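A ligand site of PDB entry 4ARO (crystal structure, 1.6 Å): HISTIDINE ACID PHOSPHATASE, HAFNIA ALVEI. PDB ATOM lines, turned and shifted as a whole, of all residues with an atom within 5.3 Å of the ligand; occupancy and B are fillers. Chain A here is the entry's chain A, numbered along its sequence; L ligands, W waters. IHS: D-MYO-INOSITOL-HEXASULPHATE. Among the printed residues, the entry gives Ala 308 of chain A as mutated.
The side-chain carboxylate of Asp 307 lies within salt-bridge range of the guanidinium group of Arg 18, 3.3 Å away. A ring nitrogen (NE2) of His 306 sits at hydrogen-bond distance from the side-chain carboxylate (OD2) of Asp 90. The side-chain carboxylate of Asp 92 lies within salt-bridge range of the guanidinium group of Arg 94. The guanidinium group (NE) of Arg 18 is in hydrogen-bond range of a ring nitrogen (NE2) of His 19. The guanidinium group of Arg 18 lies within salt-bridge range of the side-chain carboxylate of Glu 222 (2.8 Å). The backbone NH (N) of His 19 sits at hydrogen-bond distance from the backbone carbonyl oxygen (O) of Gly 305.
Asp 92 touches the ligand (OD2 to O4, 3.98 Å). Glu 222 touches the ligand (CG to O25, 3.6 Å). His 253 touches the ligand. Phe 257 touches the ligand. The nearest printed residue that does not touch the ligand is Ala 308 (4.5 Å).
Water W8 lies within hydrogen-bond range of O42 of the ligand (2.5 Å) and OG1 of Thr 25 (2.8 Å). Water W7 bridges O35 of the ligand (2.7 Å) and O of Thr 219 (3.0 Å). Water W3 lies within hydrogen-bond range of the side-chain carboxylate of Asp 307 (2.4 Å), an oxygen (O2) of the ligand (2.7 Å) and the backbone NH of Ala 308 (3.0 Å). Water W9 lies within hydrogen-bond range of the side-chain hydroxyl of Ser 218 (2.9 Å), the side-chain amide oxygen of Gln 256 (2.9 Å), an oxygen (O35) of the ligand (3.0 Å) and a ring nitrogen (NE2) of His 253 (3.4 Å). Water W5 bridges O45 of the ligand and NE2 of Gln 256. Water W4 bridges NH1 of Arg 94 and O22 of the ligand.
O36 of the ligand sits at hydrogen-bond distance from N of Asp 307. The side-chain carboxylate (OD2) of Asp 307 sits close to an oxygen (O25) of the ligand (2.4 Å). OG1 of Thr 219 is in hydrogen-bond range of O44 of the ligand (2.6 Å). An oxygen (O26) of the ligand lies within hydrogen-bond range of a ring nitrogen (ND1) of His 306. NE of Arg 22 is in salt-bridge range of O46 of the ligand (2.8 Å). The side-chain amino group (NZ) of Lys 26 lies within salt-bridge range of an oxygen (O24) of the ligand (2.9 Å). NH2 of Arg 94 is in salt-bridge range of O22 of the ligand (2.9 Å). The side-chain hydroxyl of Thr 25 lies within hydrogen-bond range of an oxygen (O34) of the ligand, 2.9 Å away. An oxygen (O46) of the ligand lies within salt-bridge range of the guanidinium group (NH2) of Arg 18 (3.0 Å). An oxygen (O46) of the ligand is in hydrogen-bond range of a ring nitrogen (NE2) of His 19, 3.1 Å away. O4 of the ligand sits at hydrogen-bond distance from NE2 of His 128 (3.3 Å).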
ATOM      1  N   ARG A  18       4.576  22.318   6.789  1.00  0.00           N
ATOM      2  CA  ARG A  18       3.218  22.308   7.372  1.00  0.00           C
ATOM      3  C   ARG A  18       3.159  21.231   8.441  1.00  0.00           C
ATOM      4  O   ARG A  18       3.795  20.239   8.372  1.00  0.00           O
ATOM      5  CB  ARG A  18       2.162  22.102   6.321  1.00  0.00           C
ATOM      6  CG  ARG A  18       0.741  22.287   6.758  1.00  0.00           C
ATOM      7  CD  ARG A  18      -0.261  22.171   5.646  1.00  0.00           C
ATOM      8  NE  ARG A  18      -1.618  22.308   6.202  1.00  0.00           N
ATOM      9  CZ  ARG A  18      -2.681  21.711   5.678  1.00  0.00           C
ATOM     10  NH1 ARG A  18      -2.613  21.048   4.514  1.00  0.00           N
ATOM     11  NH2 ARG A  18      -3.822  21.798   6.270  1.00  0.00           N
ATOM     12  N   HIS A  19       2.262  21.494   9.396  1.00  0.00           N
ATOM     13  CA  HIS A  19       1.918  20.502  10.418  1.00  0.00           C
ATOM     14  C   HIS A  19       1.313  19.254   9.733  1.00  0.00           C
ATOM     15  O   HIS A  19       0.917  19.253   8.545  1.00  0.00           O
ATOM     16  CB  HIS A  19       0.846  21.092  11.352  1.00  0.00           C
ATOM     17  CG  HIS A  19      -0.406  21.418  10.631  1.00  0.00           C
ATOM     18  ND1 HIS A  19      -1.325  20.463  10.254  1.00  0.00           N
ATOM     19  CD2 HIS A  19      -0.848  22.574  10.126  1.00  0.00           C
ATOM     20  CE1 HIS A  19      -2.283  21.022   9.549  1.00  0.00           C
ATOM     21  NE2 HIS A  19      -2.002  22.296   9.432  1.00  0.00           N
ATOM     22  N   ARG A  22      -4.525  16.592  10.669  1.00  0.00           N
ATOM     23  CA  ARG A  22      -5.259  17.195  11.791  1.00  0.00           C
ATOM     24  C   ARG A  22      -6.772  17.001  11.565  1.00  0.00           C
ATOM     25  O   ARG A  22      -7.268  16.843  10.427  1.00  0.00           O
ATOM     26  CB  ARG A  22      -4.972  18.680  11.882  1.00  0.00           C
ATOM     27  CG  ARG A  22      -5.375  19.480  10.649  1.00  0.00           C
ATOM     28  CD  ARG A  22      -5.539  20.950  10.953  1.00  0.00           C
ATOM     29  NE  ARG A  22      -5.802  21.772   9.775  1.00  0.00           N
ATOM     30  CZ  ARG A  22      -6.955  21.857   9.157  1.00  0.00           C
ATOM     31  NH1 ARG A  22      -8.024  21.135   9.574  1.00  0.00           N
ATOM     32  NH2 ARG A  22      -7.103  22.638   8.080  1.00  0.00           N
ATOM     33  N   THR A  25     -10.465  22.376  11.670  1.00  0.00           N
ATOM     34  CA  THR A  25     -10.276  23.422  12.600  1.00  0.00           C
ATOM     35  C   THR A  25     -11.555  24.058  13.112  1.00  0.00           C
ATOM     36  O   THR A  25     -11.618  24.679  14.161  1.00  0.00           O
ATOM     37  CB  THR A  25      -9.365  24.534  11.996  1.00  0.00           C
ATOM     38  OG1 THR A  25      -9.910  24.852  10.709  1.00  0.00           O
ATOM     39  CG2 THR A  25      -7.975  24.059  11.862  1.00  0.00           C
ATOM     40  N   LYS A  26     -12.637  23.872  12.360  1.00  0.00           N
ATOM     41  CA  LYS A  26     -13.938  24.350  12.698  1.00  0.00           C
ATOM     42  C   LYS A  26     -14.987  23.400  12.082  1.00  0.00           C
ATOM     43  O   LYS A  26     -14.695  22.698  11.137  1.00  0.00           O
ATOM     44  CB  LYS A  26     -14.172  25.776  12.113  1.00  0.00           C
ATOM     45  CG  LYS A  26     -14.053  25.840  10.588  1.00  0.00           C
ATOM     46  CD  LYS A  26     -14.120  27.293  10.043  1.00  0.00           C
ATOM     47  CE  LYS A  26     -14.267  27.343   8.530  1.00  0.00           C
ATOM     48  NZ  LYS A  26     -13.979  28.688   8.010  1.00  0.00           N
ATOM     49  N   ASP A  90       5.156  26.958  15.722  1.00  0.00           N
ATOM     50  CA  ASP A  90       4.100  27.863  16.073  1.00  0.00           C
ATOM     51  C   ASP A  90       3.414  27.337  17.371  1.00  0.00           C
ATOM     52  O   ASP A  90       3.627  26.151  17.726  1.00  0.00           O
ATOM     53  CB  ASP A  90       3.106  27.991  14.909  1.00  0.00           C
ATOM     54  CG  ASP A  90       2.233  29.202  15.014  1.00  0.00           C
ATOM     55  OD1 ASP A  90       2.416  30.063  15.922  1.00  0.00           O
ATOM     56  OD2 ASP A  90       1.305  29.288  14.209  1.00  0.00           O
ATOM     57  N   ASP A  92       0.402  26.524  18.161  1.00  0.00           N
ATOM     58  CA  ASP A  92      -0.692  25.547  18.132  1.00  0.00           C
ATOM     59  C   ASP A  92      -0.256  24.162  18.544  1.00  0.00           C
ATOM     60  O   ASP A  92       0.887  23.767  18.332  1.00  0.00           O
ATOM     61  CB  ASP A  92      -1.245  25.440  16.693  1.00  0.00           C
ATOM     62  CG  ASP A  92      -1.944  26.680  16.272  1.00  0.00           C
ATOM     63  OD1 ASP A  92      -2.357  27.513  17.125  1.00  0.00           O
ATOM     64  OD2 ASP A  92      -2.231  26.772  15.042  1.00  0.00           O
ATOM     65  N   ARG A  94      -1.037  21.565  16.955  1.00  0.00           N
ATOM     66  CA  ARG A  94      -0.727  20.815  15.770  1.00  0.00           C
ATOM     67  C   ARG A  94       0.712  21.044  15.277  1.00  0.00           C
ATOM     68  O   ARG A  94       1.362  20.135  14.763  1.00  0.00           O
ATOM     69  CB  ARG A  94      -1.707  20.998  14.661  1.00  0.00           C
ATOM     70  CG  ARG A  94      -1.894  22.430  14.131  1.00  0.00           C
ATOM     71  CD  ARG A  94      -2.971  22.391  13.055  1.00  0.00           C
ATOM     72  NE  ARG A  94      -3.356  23.714  12.495  1.00  0.00           N
ATOM     73  CZ  ARG A  94      -4.212  24.529  13.077  1.00  0.00           C
ATOM     74  NH1 ARG A  94      -4.856  24.173  14.234  1.00  0.00           N
ATOM     75  NH2 ARG A  94      -4.511  25.703  12.538  1.00  0.00           N
ATOM     76  N   HIS A 128       2.226  34.866  11.889  1.00  0.00           N
ATOM     77  CA  HIS A 128       1.009  35.625  11.656  1.00  0.00           C
ATOM     78  C   HIS A 128       1.236  37.106  12.025  1.00  0.00           C
ATOM     79  O   HIS A 128       0.682  37.600  12.974  1.00  0.00           O
ATOM     80  CB  HIS A 128      -0.133  35.079  12.509  1.00  0.00           C
ATOM     81  CG  HIS A 128      -0.325  33.602  12.343  1.00  0.00           C
ATOM     82  ND1 HIS A 128       0.094  32.693  13.281  1.00  0.00           N
ATOM     83  CD2 HIS A 128      -0.887  32.885  11.340  1.00  0.00           C
ATOM     84  CE1 HIS A 128      -0.188  31.472  12.861  1.00  0.00           C
ATOM     85  NE2 HIS A 128      -0.775  31.566  11.677  1.00  0.00           N
ATOM     86  N   SER A 218     -13.298  25.035  -0.770  1.00  0.00           N
ATOM     87  CA  SER A 218     -11.886  24.944  -0.424  1.00  0.00           C
ATOM     88  C   SER A 218     -11.724  24.285   0.936  1.00  0.00           C
ATOM     89  O   SER A 218     -10.992  23.327   1.073  1.00  0.00           O
ATOM     90  CB  SER A 218     -11.204  26.287  -0.458  1.00  0.00           C
ATOM     91  OG  SER A 218      -9.919  26.206   0.209  1.00  0.00           O
ATOM     92  N   THR A 219     -12.461  24.781   1.947  1.00  0.00           N
ATOM     93  CA  THR A 219     -12.377  24.197   3.259  1.00  0.00           C
ATOM     94  C   THR A 219     -12.798  22.741   3.254  1.00  0.00           C
ATOM     95  O   THR A 219     -12.133  21.819   3.827  1.00  0.00           O
ATOM     96  CB  THR A 219     -13.278  25.001   4.187  1.00  0.00           C
ATOM     97  OG1 THR A 219     -12.825  26.352   4.252  1.00  0.00           O
ATOM     98  CG2 THR A 219     -13.311  24.381   5.586  1.00  0.00           C
ATOM     99  N   GLU A 222     -10.363  20.232   1.531  1.00  0.00           N
ATOM    100  CA  GLU A 222      -9.194  19.997   2.387  1.00  0.00           C
ATOM    101  C   GLU A 222      -9.579  19.001   3.504  1.00  0.00           C
ATOM    102  O   GLU A 222      -8.808  18.135   3.816  1.00  0.00           O
ATOM    103  CB  GLU A 222      -8.627  21.288   3.001  1.00  0.00           C
ATOM    104  CG  GLU A 222      -7.497  21.109   4.007  1.00  0.00           C
ATOM    105  CD  GLU A 222      -6.226  20.646   3.407  1.00  0.00           C
ATOM    106  OE1 GLU A 222      -6.098  20.610   2.088  1.00  0.00           O
ATOM    107  OE2 GLU A 222      -5.298  20.307   4.211  1.00  0.00           O
ATOM    108  N   HIS A 253      -9.341  24.511  -3.437  1.00  0.00           N
ATOM    109  CA  HIS A 253      -8.459  24.814  -2.282  1.00  0.00           C
ATOM    110  C   HIS A 253      -7.207  25.523  -2.727  1.00  0.00           C
ATOM    111  O   HIS A 253      -6.813  26.582  -2.186  1.00  0.00           O
ATOM    112  CB  HIS A 253      -8.196  23.516  -1.478  1.00  0.00           C
ATOM    113  CG  HIS A 253      -7.417  23.746  -0.214  1.00  0.00           C
ATOM    114  ND1 HIS A 253      -6.080  23.434  -0.061  1.00  0.00           N
ATOM    115  CD2 HIS A 253      -7.803  24.297   0.947  1.00  0.00           C
ATOM    116  CE1 HIS A 253      -5.703  23.768   1.153  1.00  0.00           C
ATOM    117  NE2 HIS A 253      -6.725  24.333   1.770  1.00  0.00           N
ATOM    118  N   GLN A 256      -8.156  29.091  -3.730  1.00  0.00           N
ATOM    119  CA  GLN A 256      -8.377  30.004  -2.626  1.00  0.00           C
ATOM    120  C   GLN A 256      -7.016  30.467  -1.998  1.00  0.00           C
ATOM    121  O   GLN A 256      -6.853  31.640  -1.651  1.00  0.00           O
ATOM    122  CB  GLN A 256      -9.236  29.321  -1.576  1.00  0.00           C
ATOM    123  CG  GLN A 256      -9.500  30.145  -0.332  1.00  0.00           C
ATOM    124  CD  GLN A 256      -8.898  29.556   0.900  1.00  0.00           C
ATOM    125  OE1 GLN A 256      -9.004  28.345   1.172  1.00  0.00           O
ATOM    126  NE2 GLN A 256      -8.286  30.379   1.673  1.00  0.00           N
ATOM    127  N   PHE A 257      -6.078  29.529  -1.883  1.00  0.00           N
ATOM    128  CA  PHE A 257      -4.761  29.892  -1.403  1.00  0.00           C
ATOM    129  C   PHE A 257      -3.966  30.735  -2.370  1.00  0.00           C
ATOM    130  O   PHE A 257      -3.217  31.617  -1.934  1.00  0.00           O
ATOM    131  CB  PHE A 257      -4.025  28.611  -1.009  1.00  0.00           C
ATOM    132  CG  PHE A 257      -4.303  28.222   0.397  1.00  0.00           C
ATOM    133  CD1 PHE A 257      -5.527  27.697   0.778  1.00  0.00           C
ATOM    134  CD2 PHE A 257      -3.368  28.494   1.382  1.00  0.00           C
ATOM    135  CE1 PHE A 257      -5.793  27.426   2.129  1.00  0.00           C
ATOM    136  CE2 PHE A 257      -3.620  28.216   2.704  1.00  0.00           C
ATOM    137  CZ  PHE A 257      -4.827  27.712   3.101  1.00  0.00           C
ATOM    138  N   GLY A 305       4.888  25.126  10.728  1.00  0.00           N
ATOM    139  CA  GLY A 305       3.910  26.126  10.457  1.00  0.00           C
ATOM    140  C   GLY A 305       2.699  25.611   9.689  1.00  0.00           C
ATOM    141  O   GLY A 305       2.203  24.500   9.941  1.00  0.00           O
ATOM    142  N   HIS A 306       2.191  26.433   8.783  1.00  0.00           N
ATOM    143  CA  HIS A 306       0.894  26.279   8.177  1.00  0.00           C
ATOM    144  C   HIS A 306       0.921  26.350   6.681  1.00  0.00           C
ATOM    145  O   HIS A 306       1.874  26.885   6.094  1.00  0.00           O
ATOM    146  CB  HIS A 306      -0.052  27.376   8.691  1.00  0.00           C
ATOM    147  CG  HIS A 306      -0.121  27.450  10.188  1.00  0.00           C
ATOM    148  ND1 HIS A 306      -1.005  26.671  10.954  1.00  0.00           N
ATOM    149  CD2 HIS A 306       0.670  28.104  11.084  1.00  0.00           C
ATOM    150  CE1 HIS A 306      -0.761  26.898  12.247  1.00  0.00           C
ATOM    151  NE2 HIS A 306       0.250  27.739  12.342  1.00  0.00           N
ATOM    152  N   ASP A 307      -0.168  25.918   6.048  1.00  0.00           N
ATOM    153  CA  ASP A 307      -0.207  25.990   4.599  1.00  0.00           C
ATOM    154  C   ASP A 307      -0.099  27.481   4.150  1.00  0.00           C
ATOM    155  O   ASP A 307       0.508  27.745   3.140  1.00  0.00           O
ATOM    156  CB  ASP A 307      -1.402  25.264   3.986  1.00  0.00           C
ATOM    157  CG  ASP A 307      -2.688  25.489   4.661  1.00  0.00           C
ATOM    158  OD1 ASP A 307      -2.950  26.493   5.395  1.00  0.00           O
ATOM    159  OD2 ASP A 307      -3.574  24.529   4.453  1.00  0.00           O
ATOM    160  N   ALA A 308      -0.691  28.410   4.860  1.00  0.00           N
ATOM    161  CA  ALA A 308      -0.631  29.823   4.462  1.00  0.00           C
ATOM    162  C   ALA A 308       0.793  30.341   4.439  1.00  0.00           C
ATOM    163  O   ALA A 308       1.164  31.236   3.627  1.00  0.00           O
ATOM    164  CB  ALA A 308      -1.476  30.759   5.370  1.00  0.00           C
HETATM  165  C1  IHS L   1      -5.500  28.065   9.384  1.00  0.00           C
HETATM  166  O1  IHS L   1      -4.517  28.045  10.419  1.00  0.00           O
HETATM  167  S1  IHS L   1      -3.501  29.239  10.550  1.00  0.00           S
HETATM  168  C2  IHS L   1      -6.827  28.543   9.978  1.00  0.00           C
HETATM  169  O2  IHS L   1      -2.642  29.220   9.408  1.00  0.00           O
HETATM  170  S2  IHS L   1      -7.488  28.093  12.455  1.00  0.00           S
HETATM  171  C3  IHS L   1      -7.919  28.593   8.930  1.00  0.00           C
HETATM  172  O3  IHS L   1      -4.450  30.527  10.564  1.00  0.00           O
HETATM  173  S3  IHS L   1      -9.546  30.525   9.299  1.00  0.00           S
HETATM  174  C4  IHS L   1      -8.060  27.231   8.215  1.00  0.00           C
HETATM  175  O4  IHS L   1      -2.801  29.014  11.803  1.00  0.00           O
HETATM  176  S4  IHS L   1     -10.427  26.660   7.169  1.00  0.00           S
HETATM  177  C5  IHS L   1      -6.705  26.721   7.677  1.00  0.00           C
HETATM  178  S5  IHS L   1      -6.811  25.096   5.587  1.00  0.00           S
HETATM  179  C6  IHS L   1      -5.615  26.679   8.705  1.00  0.00           C
HETATM  180  S6  IHS L   1      -3.477  25.009   8.580  1.00  0.00           S
HETATM  181  O12 IHS L   1      -7.187  27.614  10.969  1.00  0.00           O
HETATM  182  O13 IHS L   1      -9.159  28.989   9.519  1.00  0.00           O
HETATM  183  O14 IHS L   1      -8.941  27.321   7.085  1.00  0.00           O
HETATM  184  O15 IHS L   1      -6.818  25.425   7.128  1.00  0.00           O
HETATM  185  O16 IHS L   1      -4.290  26.282   8.110  1.00  0.00           O
HETATM  186  O22 IHS L   1      -6.946  27.092  13.371  1.00  0.00           O
HETATM  187  O23 IHS L   1     -10.978  30.513  10.046  1.00  0.00           O
HETATM  188  O24 IHS L   1     -11.235  27.775   7.946  1.00  0.00           O
HETATM  189  O25 IHS L   1      -5.789  24.033   5.335  1.00  0.00           O
HETATM  190  O26 IHS L   1      -3.160  25.209   9.985  1.00  0.00           O
HETATM  191  O32 IHS L   1      -6.881  29.393  12.670  1.00  0.00           O
HETATM  192  O33 IHS L   1      -9.505  30.757   7.886  1.00  0.00           O
HETATM  193  O34 IHS L   1     -10.326  25.403   7.864  1.00  0.00           O
HETATM  194  O35 IHS L   1      -8.238  24.555   5.291  1.00  0.00           O
HETATM  195  O36 IHS L   1      -2.293  24.923   7.834  1.00  0.00           O
HETATM  196  O42 IHS L   1      -9.079  28.154  12.483  1.00  0.00           O
HETATM  197  O43 IHS L   1      -8.539  31.264  10.013  1.00  0.00           O
HETATM  198  O44 IHS L   1     -10.678  26.618   5.753  1.00  0.00           O
HETATM  199  O45 IHS L   1      -6.673  26.348   4.901  1.00  0.00           O
HETATM  200  O46 IHS L   1      -4.441  23.801   8.388  1.00  0.00           O
HETATM  201  O   HOH W   1     -10.209  29.141   5.123  1.00  0.00           O
HETATM  202  O   HOH W   2      -4.616  32.629  12.231  1.00  0.00           O
HETATM  203  O   HOH W   3      -3.041  28.498   6.789  1.00  0.00           O
HETATM  204  O   HOH W   4      -6.809  25.256  15.876  1.00  0.00           O
HETATM  205  O   HOH W   5      -7.716  29.122   4.537  1.00  0.00           O
HETATM  206  O   HOH W   6      -5.510  29.887   6.401  1.00  0.00           O
HETATM  207  O   HOH W   7     -10.103  22.653   5.877  1.00  0.00           O
HETATM  208  O   HOH W   8     -10.904  27.404  10.973  1.00  0.00           O
HETATM  209  O   HOH W   9      -9.323  26.101   3.001  1.00  0.00           O
HETATM  210  O   HOH W  10      -1.997  29.542  14.493  1.00  0.00           O
